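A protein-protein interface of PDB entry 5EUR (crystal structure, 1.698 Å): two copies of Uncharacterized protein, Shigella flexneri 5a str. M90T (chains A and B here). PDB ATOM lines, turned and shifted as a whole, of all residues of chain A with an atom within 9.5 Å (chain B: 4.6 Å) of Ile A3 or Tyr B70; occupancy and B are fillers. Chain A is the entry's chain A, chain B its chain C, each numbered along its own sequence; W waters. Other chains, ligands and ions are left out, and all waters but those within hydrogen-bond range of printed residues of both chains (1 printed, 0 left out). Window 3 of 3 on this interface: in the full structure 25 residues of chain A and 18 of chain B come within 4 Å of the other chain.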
ATOM      1  N   SER A   2      12.573 -14.766  24.020  1.00  0.00           N
ATOM      2  CA  SER A   2      11.265 -14.638  24.660  1.00  0.00           C
ATOM      3  C   SER A   2      10.637 -13.339  24.193  1.00  0.00           C
ATOM      4  O   SER A   2      11.343 -12.465  23.690  1.00  0.00           O
ATOM      5  CB  SER A   2      11.393 -14.662  26.184  1.00  0.00           C
ATOM      6  OG  SER A   2      11.949 -13.442  26.666  1.00  0.00           O
ATOM      7  N   ILE A   3       9.326 -13.182  24.346  1.00  0.00           N
ATOM      8  CA  ILE A   3       8.724 -11.908  23.984  1.00  0.00           C
ATOM      9  C   ILE A   3       8.803 -10.987  25.193  1.00  0.00           C
ATOM     10  O   ILE A   3       8.748 -11.433  26.347  1.00  0.00           O
ATOM     11  CB  ILE A   3       7.279 -12.073  23.477  1.00  0.00           C
ATOM     12  CG1 ILE A   3       6.367 -12.669  24.549  1.00  0.00           C
ATOM     13  CG2 ILE A   3       7.239 -12.928  22.200  1.00  0.00           C
ATOM     14  CD1 ILE A   3       4.887 -12.578  24.185  1.00  0.00           C
ATOM     15  N   SER A   4       8.998  -9.698  24.926  1.00  0.00           N
ATOM     16  CA  SER A   4       9.171  -8.758  26.017  1.00  0.00           C
ATOM     17  C   SER A   4       7.825  -8.317  26.590  1.00  0.00           C
ATOM     18  O   SER A   4       6.767  -8.414  25.956  1.00  0.00           O
ATOM     19  CB  SER A   4       9.985  -7.543  25.563  1.00  0.00           C
ATOM     20  OG  SER A   4       9.493  -7.038  24.346  1.00  0.00           O
ATOM     21  N   TYR A   5       7.891  -7.815  27.814  1.00  0.00           N
ATOM     22  CA  TYR A   5       6.769  -7.165  28.464  1.00  0.00           C
ATOM     23  C   TYR A   5       6.827  -5.674  28.186  1.00  0.00           C
ATOM     24  O   TYR A   5       7.899  -5.107  27.963  1.00  0.00           O
ATOM     25  CB  TYR A   5       6.818  -7.394  29.981  1.00  0.00           C
ATOM     26  CG  TYR A   5       6.735  -8.845  30.360  1.00  0.00           C
ATOM     27  CD1 TYR A   5       5.520  -9.408  30.749  1.00  0.00           C
ATOM     28  CD2 TYR A   5       7.859  -9.666  30.323  1.00  0.00           C
ATOM     29  CE1 TYR A   5       5.429 -10.734  31.073  1.00  0.00           C
ATOM     30  CE2 TYR A   5       7.772 -10.995  30.643  1.00  0.00           C
ATOM     31  CZ  TYR A   5       6.561 -11.523  31.022  1.00  0.00           C
ATOM     32  OH  TYR A   5       6.459 -12.845  31.349  1.00  0.00           O
ATOM     33  N   ARG A   6       5.663  -5.040  28.192  1.00  0.00           N
ATOM     34  CA  ARG A   6       5.660  -3.592  28.182  1.00  0.00           C
ATOM     35  C   ARG A   6       6.226  -3.092  29.516  1.00  0.00           C
ATOM     36  O   ARG A   6       6.427  -3.860  30.461  1.00  0.00           O
ATOM     37  CB  ARG A   6       4.242  -3.087  27.912  1.00  0.00           C
ATOM     38  CG  ARG A   6       3.789  -3.514  26.511  1.00  0.00           C
ATOM     39  CD  ARG A   6       2.456  -2.959  26.039  1.00  0.00           C
ATOM     40  NE  ARG A   6       2.170  -3.513  24.714  1.00  0.00           N
ATOM     41  CZ  ARG A   6       2.563  -2.991  23.558  1.00  0.00           C
ATOM     42  NH1 ARG A   6       3.223  -1.838  23.523  1.00  0.00           N
ATOM     43  NH2 ARG A   6       2.257  -3.616  22.429  1.00  0.00           N
ATOM     44  N   MET A  39       7.825 -14.844  35.633  1.00  0.00           N
ATOM     45  CA  MET A  39       8.135 -14.017  34.460  1.00  0.00           C
ATOM     46  C   MET A  39       9.585 -14.206  34.035  1.00  0.00           C
ATOM     47  O   MET A  39       9.890 -14.407  32.840  1.00  0.00           O
ATOM     48  CB  MET A  39       7.873 -12.536  34.758  1.00  0.00           C
ATOM     49  CG  MET A  39       6.381 -12.177  34.940  1.00  0.00           C
ATOM     50  SD  MET A  39       6.218 -10.513  35.666  1.00  0.00           S
ATOM     51  CE  MET A  39       6.947  -9.498  34.383  1.00  0.00           C
ATOM     52  N   LEU A  40      10.497 -14.127  35.015  1.00  0.00           N
ATOM     53  CA  LEU A  40      11.921 -14.242  34.718  1.00  0.00           C
ATOM     54  C   LEU A  40      12.265 -15.635  34.206  1.00  0.00           C
ATOM     55  O   LEU A  40      12.960 -15.772  33.198  1.00  0.00           O
ATOM     56  CB  LEU A  40      12.749 -13.893  35.956  1.00  0.00           C
ATOM     57  CG  LEU A  40      12.690 -12.423  36.372  1.00  0.00           C
ATOM     58  CD1 LEU A  40      13.319 -12.267  37.761  1.00  0.00           C
ATOM     59  CD2 LEU A  40      13.431 -11.532  35.344  1.00  0.00           C
ATOM     60  N   SER A  42      10.389 -17.651  32.658  1.00  0.00           N
ATOM     61  CA  SER A  42       9.841 -17.799  31.316  1.00  0.00           C
ATOM     62  C   SER A  42      10.669 -17.066  30.268  1.00  0.00           C
ATOM     63  O   SER A  42      10.537 -17.372  29.072  1.00  0.00           O
ATOM     64  CB  SER A  42       8.387 -17.327  31.294  1.00  0.00           C
ATOM     65  OG  SER A  42       8.305 -15.923  31.151  1.00  0.00           O
ATOM     66  N   THR A  43      11.527 -16.118  30.673  1.00  0.00           N
ATOM     67  CA  THR A  43      12.433 -15.553  29.664  1.00  0.00           C
ATOM     68  C   THR A  43      13.552 -16.507  29.250  1.00  0.00           C
ATOM     69  O   THR A  43      14.184 -16.271  28.217  1.00  0.00           O
ATOM     70  CB  THR A  43      13.079 -14.235  30.132  1.00  0.00           C
ATOM     71  OG1 THR A  43      14.088 -14.496  31.122  1.00  0.00           O
ATOM     72  CG2 THR A  43      12.033 -13.281  30.682  1.00  0.00           C
ATOM     73  N   GLY A  44      13.805 -17.579  29.996  1.00  0.00           N
ATOM     74  CA  GLY A  44      14.882 -18.488  29.639  1.00  0.00           C
ATOM     75  C   GLY A  44      16.253 -17.851  29.764  1.00  0.00           C
ATOM     76  O   GLY A  44      16.648 -17.439  30.855  1.00  0.00           O
ATOM     77  N   ASP A  46      17.101 -15.153  27.767  1.00  0.00           N
ATOM     78  CA  ASP A  46      16.937 -13.875  27.084  1.00  0.00           C
ATOM     79  C   ASP A  46      17.240 -12.751  28.074  1.00  0.00           C
ATOM     80  O   ASP A  46      16.352 -12.096  28.635  1.00  0.00           O
ATOM     81  CB  ASP A  46      15.532 -13.787  26.506  1.00  0.00           C
ATOM     82  CG  ASP A  46      15.333 -12.598  25.624  1.00  0.00           C
ATOM     83  OD1 ASP A  46      16.246 -11.752  25.510  1.00  0.00           O
ATOM     84  OD2 ASP A  46      14.243 -12.524  25.029  1.00  0.00           O
ATOM     85  N   ALA A  48      18.383  -9.770  27.756  1.00  0.00           N
ATOM     86  CA  ALA A  48      17.864  -8.434  27.482  1.00  0.00           C
ATOM     87  C   ALA A  48      16.468  -8.263  28.072  1.00  0.00           C
ATOM     88  O   ALA A  48      16.157  -7.232  28.691  1.00  0.00           O
ATOM     89  CB  ALA A  48      17.855  -8.177  25.975  1.00  0.00           C
ATOM     90  N   ASN A  49      15.623  -9.284  27.916  1.00  0.00           N
ATOM     91  CA  ASN A  49      14.266  -9.211  28.446  1.00  0.00           C
ATOM     92  C   ASN A  49      14.277  -9.231  29.967  1.00  0.00           C
ATOM     93  O   ASN A  49      13.564  -8.445  30.614  1.00  0.00           O
ATOM     94  CB  ASN A  49      13.417 -10.369  27.902  1.00  0.00           C
ATOM     95  CG  ASN A  49      11.929 -10.153  28.113  1.00  0.00           C
ATOM     96  OD1 ASN A  49      11.499  -9.097  28.578  1.00  0.00           O
ATOM     97  ND2 ASN A  49      11.126 -11.162  27.767  1.00  0.00           N
ATOM     98  N   SER A  50      15.068 -10.131  30.560  1.00  0.00           N
ATOM     99  CA  SER A  50      15.083 -10.182  32.021  1.00  0.00           C
ATOM    100  C   SER A  50      15.670  -8.900  32.602  1.00  0.00           C
ATOM    101  O   SER A  50      15.233  -8.440  33.664  1.00  0.00           O
ATOM    102  CB  SER A  50      15.823 -11.426  32.531  1.00  0.00           C
ATOM    103  OG  SER A  50      17.168 -11.528  32.084  1.00  0.00           O
ATOM    104  N   ARG A  52      15.218  -5.907  31.306  1.00  0.00           N
ATOM    105  CA  ARG A  52      14.095  -4.968  31.283  1.00  0.00           C
ATOM    106  C   ARG A  52      13.163  -5.182  32.473  1.00  0.00           C
ATOM    107  O   ARG A  52      12.784  -4.230  33.181  1.00  0.00           O
ATOM    108  CB  ARG A  52      13.305  -5.111  29.976  1.00  0.00           C
ATOM    109  CG  ARG A  52      13.921  -4.451  28.751  1.00  0.00           C
ATOM    110  CD  ARG A  52      13.036  -4.695  27.507  1.00  0.00           C
ATOM    111  NE  ARG A  52      11.643  -4.298  27.735  1.00  0.00           N
ATOM    112  CZ  ARG A  52      11.126  -3.111  27.422  1.00  0.00           C
ATOM    113  NH1 ARG A  52      11.877  -2.184  26.847  1.00  0.00           N
ATOM    114  NH2 ARG A  52       9.849  -2.853  27.679  1.00  0.00           N
ATOM    115  N   ILE A  53      12.745  -6.435  32.682  1.00  0.00           N
ATOM    116  CA  ILE A  53      11.859  -6.738  33.802  1.00  0.00           C
ATOM    117  C   ILE A  53      12.454  -6.226  35.107  1.00  0.00           C
ATOM    118  O   ILE A  53      11.781  -5.555  35.899  1.00  0.00           O
ATOM    119  CB  ILE A  53      11.596  -8.250  33.877  1.00  0.00           C
ATOM    120  CG1 ILE A  53      10.770  -8.705  32.670  1.00  0.00           C
ATOM    121  CG2 ILE A  53      10.875  -8.588  35.160  1.00  0.00           C
ATOM    122  CD1 ILE A  53      10.826 -10.225  32.461  1.00  0.00           C
ATOM    123  N   THR B  37       1.280 -13.131  28.510  1.00  0.00           N
ATOM    124  CA  THR B  37       2.659 -13.071  28.040  1.00  0.00           C
ATOM    125  C   THR B  37       3.507 -14.140  28.716  1.00  0.00           C
ATOM    126  O   THR B  37       4.322 -14.799  28.057  1.00  0.00           O
ATOM    127  CB  THR B  37       3.244 -11.684  28.320  1.00  0.00           C
ATOM    128  OG1 THR B  37       2.412 -10.680  27.721  1.00  0.00           O
ATOM    129  CG2 THR B  37       4.665 -11.573  27.759  1.00  0.00           C
ATOM    130  N   LEU B  40       2.630 -17.742  27.502  1.00  0.00           N
ATOM    131  CA  LEU B  40       3.189 -17.998  26.177  1.00  0.00           C
ATOM    132  C   LEU B  40       4.701 -18.196  26.252  1.00  0.00           C
ATOM    133  O   LEU B  40       5.234 -19.152  25.685  1.00  0.00           O
ATOM    134  CB  LEU B  40       2.853 -16.846  25.232  1.00  0.00           C
ATOM    135  CG  LEU B  40       1.376 -16.750  24.879  1.00  0.00           C
ATOM    136  CD1 LEU B  40       1.093 -15.430  24.171  1.00  0.00           C
ATOM    137  CD2 LEU B  40       0.982 -17.940  23.979  1.00  0.00           C
ATOM    138  N   ASN B  41       5.405 -17.290  26.945  1.00  0.00           N
ATOM    139  CA  ASN B  41       6.853 -17.450  27.099  1.00  0.00           C
ATOM    140  C   ASN B  41       7.198 -18.802  27.704  1.00  0.00           C
ATOM    141  O   ASN B  41       8.181 -19.435  27.299  1.00  0.00           O
ATOM    142  CB  ASN B  41       7.438 -16.332  27.969  1.00  0.00           C
ATOM    143  CG  ASN B  41       7.752 -15.072  27.174  1.00  0.00           C
ATOM    144  OD1 ASN B  41       7.898 -15.121  25.963  1.00  0.00           O
ATOM    145  ND2 ASN B  41       7.891 -13.943  27.870  1.00  0.00           N
ATOM    146  N   THR B  43       5.767 -21.520  27.235  1.00  0.00           N
ATOM    147  CA  THR B  43       5.736 -22.595  26.240  1.00  0.00           C
ATOM    148  C   THR B  43       7.027 -22.740  25.436  1.00  0.00           C
ATOM    149  O   THR B  43       7.182 -23.749  24.742  1.00  0.00           O
ATOM    150  CB  THR B  43       4.568 -22.435  25.250  1.00  0.00           C
ATOM    151  OG1 THR B  43       4.836 -21.363  24.325  1.00  0.00           O
ATOM    152  CG2 THR B  43       3.285 -22.193  26.013  1.00  0.00           C
ATOM    153  N   GLY B  44       7.945 -21.782  25.488  1.00  0.00           N
ATOM    154  CA  GLY B  44       9.145 -21.865  24.677  1.00  0.00           C
ATOM    155  C   GLY B  44       8.829 -21.764  23.198  1.00  0.00           C
ATOM    156  O   GLY B  44       8.270 -20.760  22.751  1.00  0.00           O
ATOM    157  N   SER B  50       1.129 -22.869  22.263  1.00  0.00           N
ATOM    158  CA  SER B  50       0.853 -21.435  22.159  1.00  0.00           C
ATOM    159  C   SER B  50      -0.301 -21.153  21.199  1.00  0.00           C
ATOM    160  O   SER B  50      -1.094 -20.238  21.445  1.00  0.00           O
ATOM    161  CB  SER B  50       2.110 -20.639  21.773  1.00  0.00           C
ATOM    162  OG  SER B  50       2.714 -21.067  20.571  1.00  0.00           O
ATOM    163  N   LEU B  54      -3.612 -18.998  22.203  1.00  0.00           N
ATOM    164  CA  LEU B  54      -4.038 -17.809  21.474  1.00  0.00           C
ATOM    165  C   LEU B  54      -5.416 -18.000  20.844  1.00  0.00           C
ATOM    166  O   LEU B  54      -6.177 -17.034  20.717  1.00  0.00           O
ATOM    167  CB  LEU B  54      -2.981 -17.431  20.435  1.00  0.00           C
ATOM    168  CG  LEU B  54      -1.724 -16.822  21.086  1.00  0.00           C
ATOM    169  CD1 LEU B  54      -0.594 -16.564  20.058  1.00  0.00           C
ATOM    170  CD2 LEU B  54      -2.050 -15.531  21.864  1.00  0.00           C
ATOM    171  N   TYR B  67       1.354 -10.624  20.769  1.00  0.00           N
ATOM    172  CA  TYR B  67       2.365 -11.462  21.415  1.00  0.00           C
ATOM    173  C   TYR B  67       3.462 -11.897  20.442  1.00  0.00           C
ATOM    174  O   TYR B  67       3.920 -13.050  20.457  1.00  0.00           O
ATOM    175  CB  TYR B  67       1.703 -12.659  22.096  1.00  0.00           C
ATOM    176  CG  TYR B  67       0.674 -12.175  23.100  1.00  0.00           C
ATOM    177  CD1 TYR B  67       1.076 -11.704  24.354  1.00  0.00           C
ATOM    178  CD2 TYR B  67      -0.677 -12.135  22.780  1.00  0.00           C
ATOM    179  CE1 TYR B  67       0.152 -11.229  25.268  1.00  0.00           C
ATOM    180  CE2 TYR B  67      -1.614 -11.668  23.689  1.00  0.00           C
ATOM    181  CZ  TYR B  67      -1.192 -11.225  24.928  1.00  0.00           C
ATOM    182  OH  TYR B  67      -2.120 -10.752  25.819  1.00  0.00           O
ATOM    183  N   GLY B  68       3.927 -10.957  19.610  1.00  0.00           N
ATOM    184  CA  GLY B  68       5.157 -11.173  18.857  1.00  0.00           C
ATOM    185  C   GLY B  68       5.183 -12.482  18.098  1.00  0.00           C
ATOM    186  O   GLY B  68       4.228 -12.837  17.399  1.00  0.00           O
ATOM    187  N   LYS B  69       6.279 -13.228  18.248  1.00  0.00           N
ATOM    188  CA  LYS B  69       6.444 -14.457  17.474  1.00  0.00           C
ATOM    189  C   LYS B  69       5.283 -15.423  17.686  1.00  0.00           C
ATOM    190  O   LYS B  69       4.854 -16.097  16.747  1.00  0.00           O
ATOM    191  CB  LYS B  69       7.787 -15.110  17.812  1.00  0.00           C
ATOM    192  CG  LYS B  69       7.886 -15.696  19.233  1.00  0.00           C
ATOM    193  CD  LYS B  69       9.266 -16.305  19.517  1.00  0.00           C
ATOM    194  CE  LYS B  69       9.372 -16.752  20.975  1.00  0.00           C
ATOM    195  NZ  LYS B  69      10.730 -17.342  21.318  1.00  0.00           N
ATOM    196  N   TYR B  70       4.740 -15.487  18.904  1.00  0.00           N
ATOM    197  CA  TYR B  70       3.627 -16.398  19.148  1.00  0.00           C
ATOM    198  C   TYR B  70       2.425 -15.988  18.322  1.00  0.00           C
ATOM    199  O   TYR B  70       1.745 -16.839  17.736  1.00  0.00           O
ATOM    200  CB  TYR B  70       3.273 -16.421  20.639  1.00  0.00           C
ATOM    201  CG  TYR B  70       4.419 -16.930  21.483  1.00  0.00           C
ATOM    202  CD1 TYR B  70       4.758 -18.285  21.477  1.00  0.00           C
ATOM    203  CD2 TYR B  70       5.168 -16.070  22.263  1.00  0.00           C
ATOM    204  CE1 TYR B  70       5.825 -18.764  22.249  1.00  0.00           C
ATOM    205  CE2 TYR B  70       6.243 -16.539  23.038  1.00  0.00           C
ATOM    206  CZ  TYR B  70       6.564 -17.876  23.012  1.00  0.00           C
ATOM    207  OH  TYR B  70       7.631 -18.336  23.770  1.00  0.00           O
ATOM    208  N   SER B  71       2.186 -14.673  18.227  1.00  0.00           N
ATOM    209  CA  SER B  71       1.085 -14.204  17.390  1.00  0.00           C
ATOM    210  C   SER B  71       1.332 -14.481  15.913  1.00  0.00           C
ATOM    211  O   SER B  71       0.387 -14.793  15.170  1.00  0.00           O
ATOM    212  CB  SER B  71       0.861 -12.719  17.620  1.00  0.00           C
ATOM    213  OG  SER B  71       0.370 -12.540  18.932  1.00  0.00           O
ATOM    214  N   ARG B  72       2.581 -14.331  15.464  1.00  0.00           N
ATOM    215  CA  ARG B  72       2.899 -14.558  14.055  1.00  0.00           C
ATOM    216  C   ARG B  72       2.700 -16.020  13.679  1.00  0.00           C
ATOM    217  O   ARG B  72       2.122 -16.323  12.627  1.00  0.00           O
ATOM    218  CB  ARG B  72       4.332 -14.118  13.758  1.00  0.00           C
ATOM    219  CG  ARG B  72       4.674 -12.697  14.177  1.00  0.00           C
ATOM    220  CD  ARG B  72       3.896 -11.647  13.398  1.00  0.00           C
ATOM    221  NE  ARG B  72       2.621 -11.288  14.023  1.00  0.00           N
ATOM    222  CZ  ARG B  72       2.486 -10.437  15.041  1.00  0.00           C
ATOM    223  NH1 ARG B  72       3.553  -9.841  15.572  1.00  0.00           N
ATOM    224  NH2 ARG B  72       1.274 -10.173  15.528  1.00  0.00           N
ATOM    225  N   TRP B  73       3.187 -16.941  14.524  1.00  0.00           N
ATOM    226  CA  TRP B  73       2.932 -18.366  14.324  1.00  0.00           C
ATOM    227  C   TRP B  73       1.439 -18.641  14.291  1.00  0.00           C
ATOM    228  O   TRP B  73       0.948 -19.373  13.425  1.00  0.00           O
ATOM    229  CB  TRP B  73       3.576 -19.183  15.449  1.00  0.00           C
ATOM    230  CG  TRP B  73       5.044 -19.039  15.550  1.00  0.00           C
ATOM    231  CD1 TRP B  73       5.904 -18.574  14.594  1.00  0.00           C
ATOM    232  CD2 TRP B  73       5.838 -19.294  16.718  1.00  0.00           C
ATOM    233  NE1 TRP B  73       7.193 -18.570  15.092  1.00  0.00           N
ATOM    234  CE2 TRP B  73       7.171 -19.002  16.392  1.00  0.00           C
ATOM    235  CE3 TRP B  73       5.542 -19.772  18.005  1.00  0.00           C
ATOM    236  CZ2 TRP B  73       8.218 -19.140  17.321  1.00  0.00           C
ATOM    237  CZ3 TRP B  73       6.574 -19.918  18.916  1.00  0.00           C
ATOM    238  CH2 TRP B  73       7.896 -19.607  18.569  1.00  0.00           C
ATOM    239  N   TRP B  74       0.702 -18.070  15.252  1.00  0.00           N
ATOM    240  CA  TRP B  74      -0.727 -18.335  15.350  1.00  0.00           C
ATOM    241  C   TRP B  74      -1.483 -17.835  14.120  1.00  0.00           C
ATOM    242  O   TRP B  74      -2.393 -18.508  13.630  1.00  0.00           O
ATOM    243  CB  TRP B  74      -1.276 -17.684  16.621  1.00  0.00           C
ATOM    244  CG  TRP B  74      -2.767 -17.637  16.682  1.00  0.00           C
ATOM    245  CD1 TRP B  74      -3.608 -18.665  16.984  1.00  0.00           C
ATOM    246  CD2 TRP B  74      -3.596 -16.492  16.443  1.00  0.00           C
ATOM    247  NE1 TRP B  74      -4.916 -18.233  16.945  1.00  0.00           N
ATOM    248  CE2 TRP B  74      -4.933 -16.902  16.624  1.00  0.00           C
ATOM    249  CE3 TRP B  74      -3.338 -15.162  16.102  1.00  0.00           C
ATOM    250  CZ2 TRP B  74      -6.009 -16.024  16.465  1.00  0.00           C
ATOM    251  CZ3 TRP B  74      -4.408 -14.293  15.942  1.00  0.00           C
ATOM    252  CH2 TRP B  74      -5.722 -14.730  16.128  1.00  0.00           C
HETATM  253  O   HOH W   1      11.015 -18.319  26.523  1.00  0.00           O
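The side-chain amide oxygen (OD1) of Asn B41 sits at hydrogen-bond distance from the backbone NH (N) of Ile A3, 2.9 Å away.
OD2 of Asp A46 sits at hydrogen-bond distance from OG of Ser A2 (3.0 Å). The side-chain hydroxyl (OG) of Ser A2 sits at hydrogen-bond distance from the side-chain amide nitrogen (ND2) of Asn A49 (2.7 Å). NH2 of Arg A52 is in hydrogen-bond range of O of Tyr A5. The backbone carbonyl oxygen (O) of Leu B40 lies within hydrogen-bond range of the side-chain hydroxyl (OH) of Tyr B70 (3.2 Å). OH of Tyr B70 is in hydrogen-bond range of O of Gly B44. The side-chain hydroxyl of Ser B71 sits at hydrogen-bond distance from the backbone NH of Tyr B67.
Among the printed residues, merely in contact across the chains: Ser A42 with Asn B41 (3.3 Å), Tyr A5 with Thr B37 (3.5 Å), Ser A2 with Asn B41 (3.5 Å), Ile A3 with Thr B37 (3.7 Å), Ile A3 with Tyr B67 (3.8 Å), Ile A3 with Tyr B70 (3.8 Å) and Tyr A5 with Asn B41 (3.9 Å).
Tyr B70 touches one residue of chain A. Of chain A, only Ser A2 (3.5 Å), Ile A3 (2.9 Å), Tyr A5 (3.9 Å) and Ser A42 (3.3 Å) come within 4 Å of Asn B41. No residue of chain A comes within 4 Å of Gly B44. Gly B68 touches none of the printed residues of chain A. Of the printed residues of chain A, Tyr B67 touches Ile A3. Of the printed residues of chain A, Thr B37 touches Ile A3 and Tyr A5. Printed residues of chain B within 4 Å of Ser A2: Asn B41 (3.5 Å). Arg B72 touches none of the printed residues of chain A. Trp B74 touches none of the printed residues of chain A. The nearest residue of chain B that does not touch Ile A3 is Lys B69 (4.1 Å). The nearest residue of chain A that does not touch Tyr B70 is Ser A2 (5.3 Å). The nearest printed residue of chain A that does not touch Tyr B67 is Ser A4 (6.8 Å).
Of the 15 printed residues of chain B, 4 touch a printed residue of chain A. Hydrophobic or aromatic side chains of chain B within 4 Å of the printed part of chain A: Tyr B67 and Tyr B70. Hydrophobic or aromatic side chains of chain A within 4 Å of the printed part of chain B: Ile A3 and Tyr A5. Among the printed residues, 8 pairs touch across the chains.
Positions printed for both chains: 40, 43, 44 and 50.
Water W1 bridges the backbone carbonyl oxygen (O) of Ser A42 (2.8 Å) and the backbone carbonyl oxygen (O) of Asn B41 (3.1 Å).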
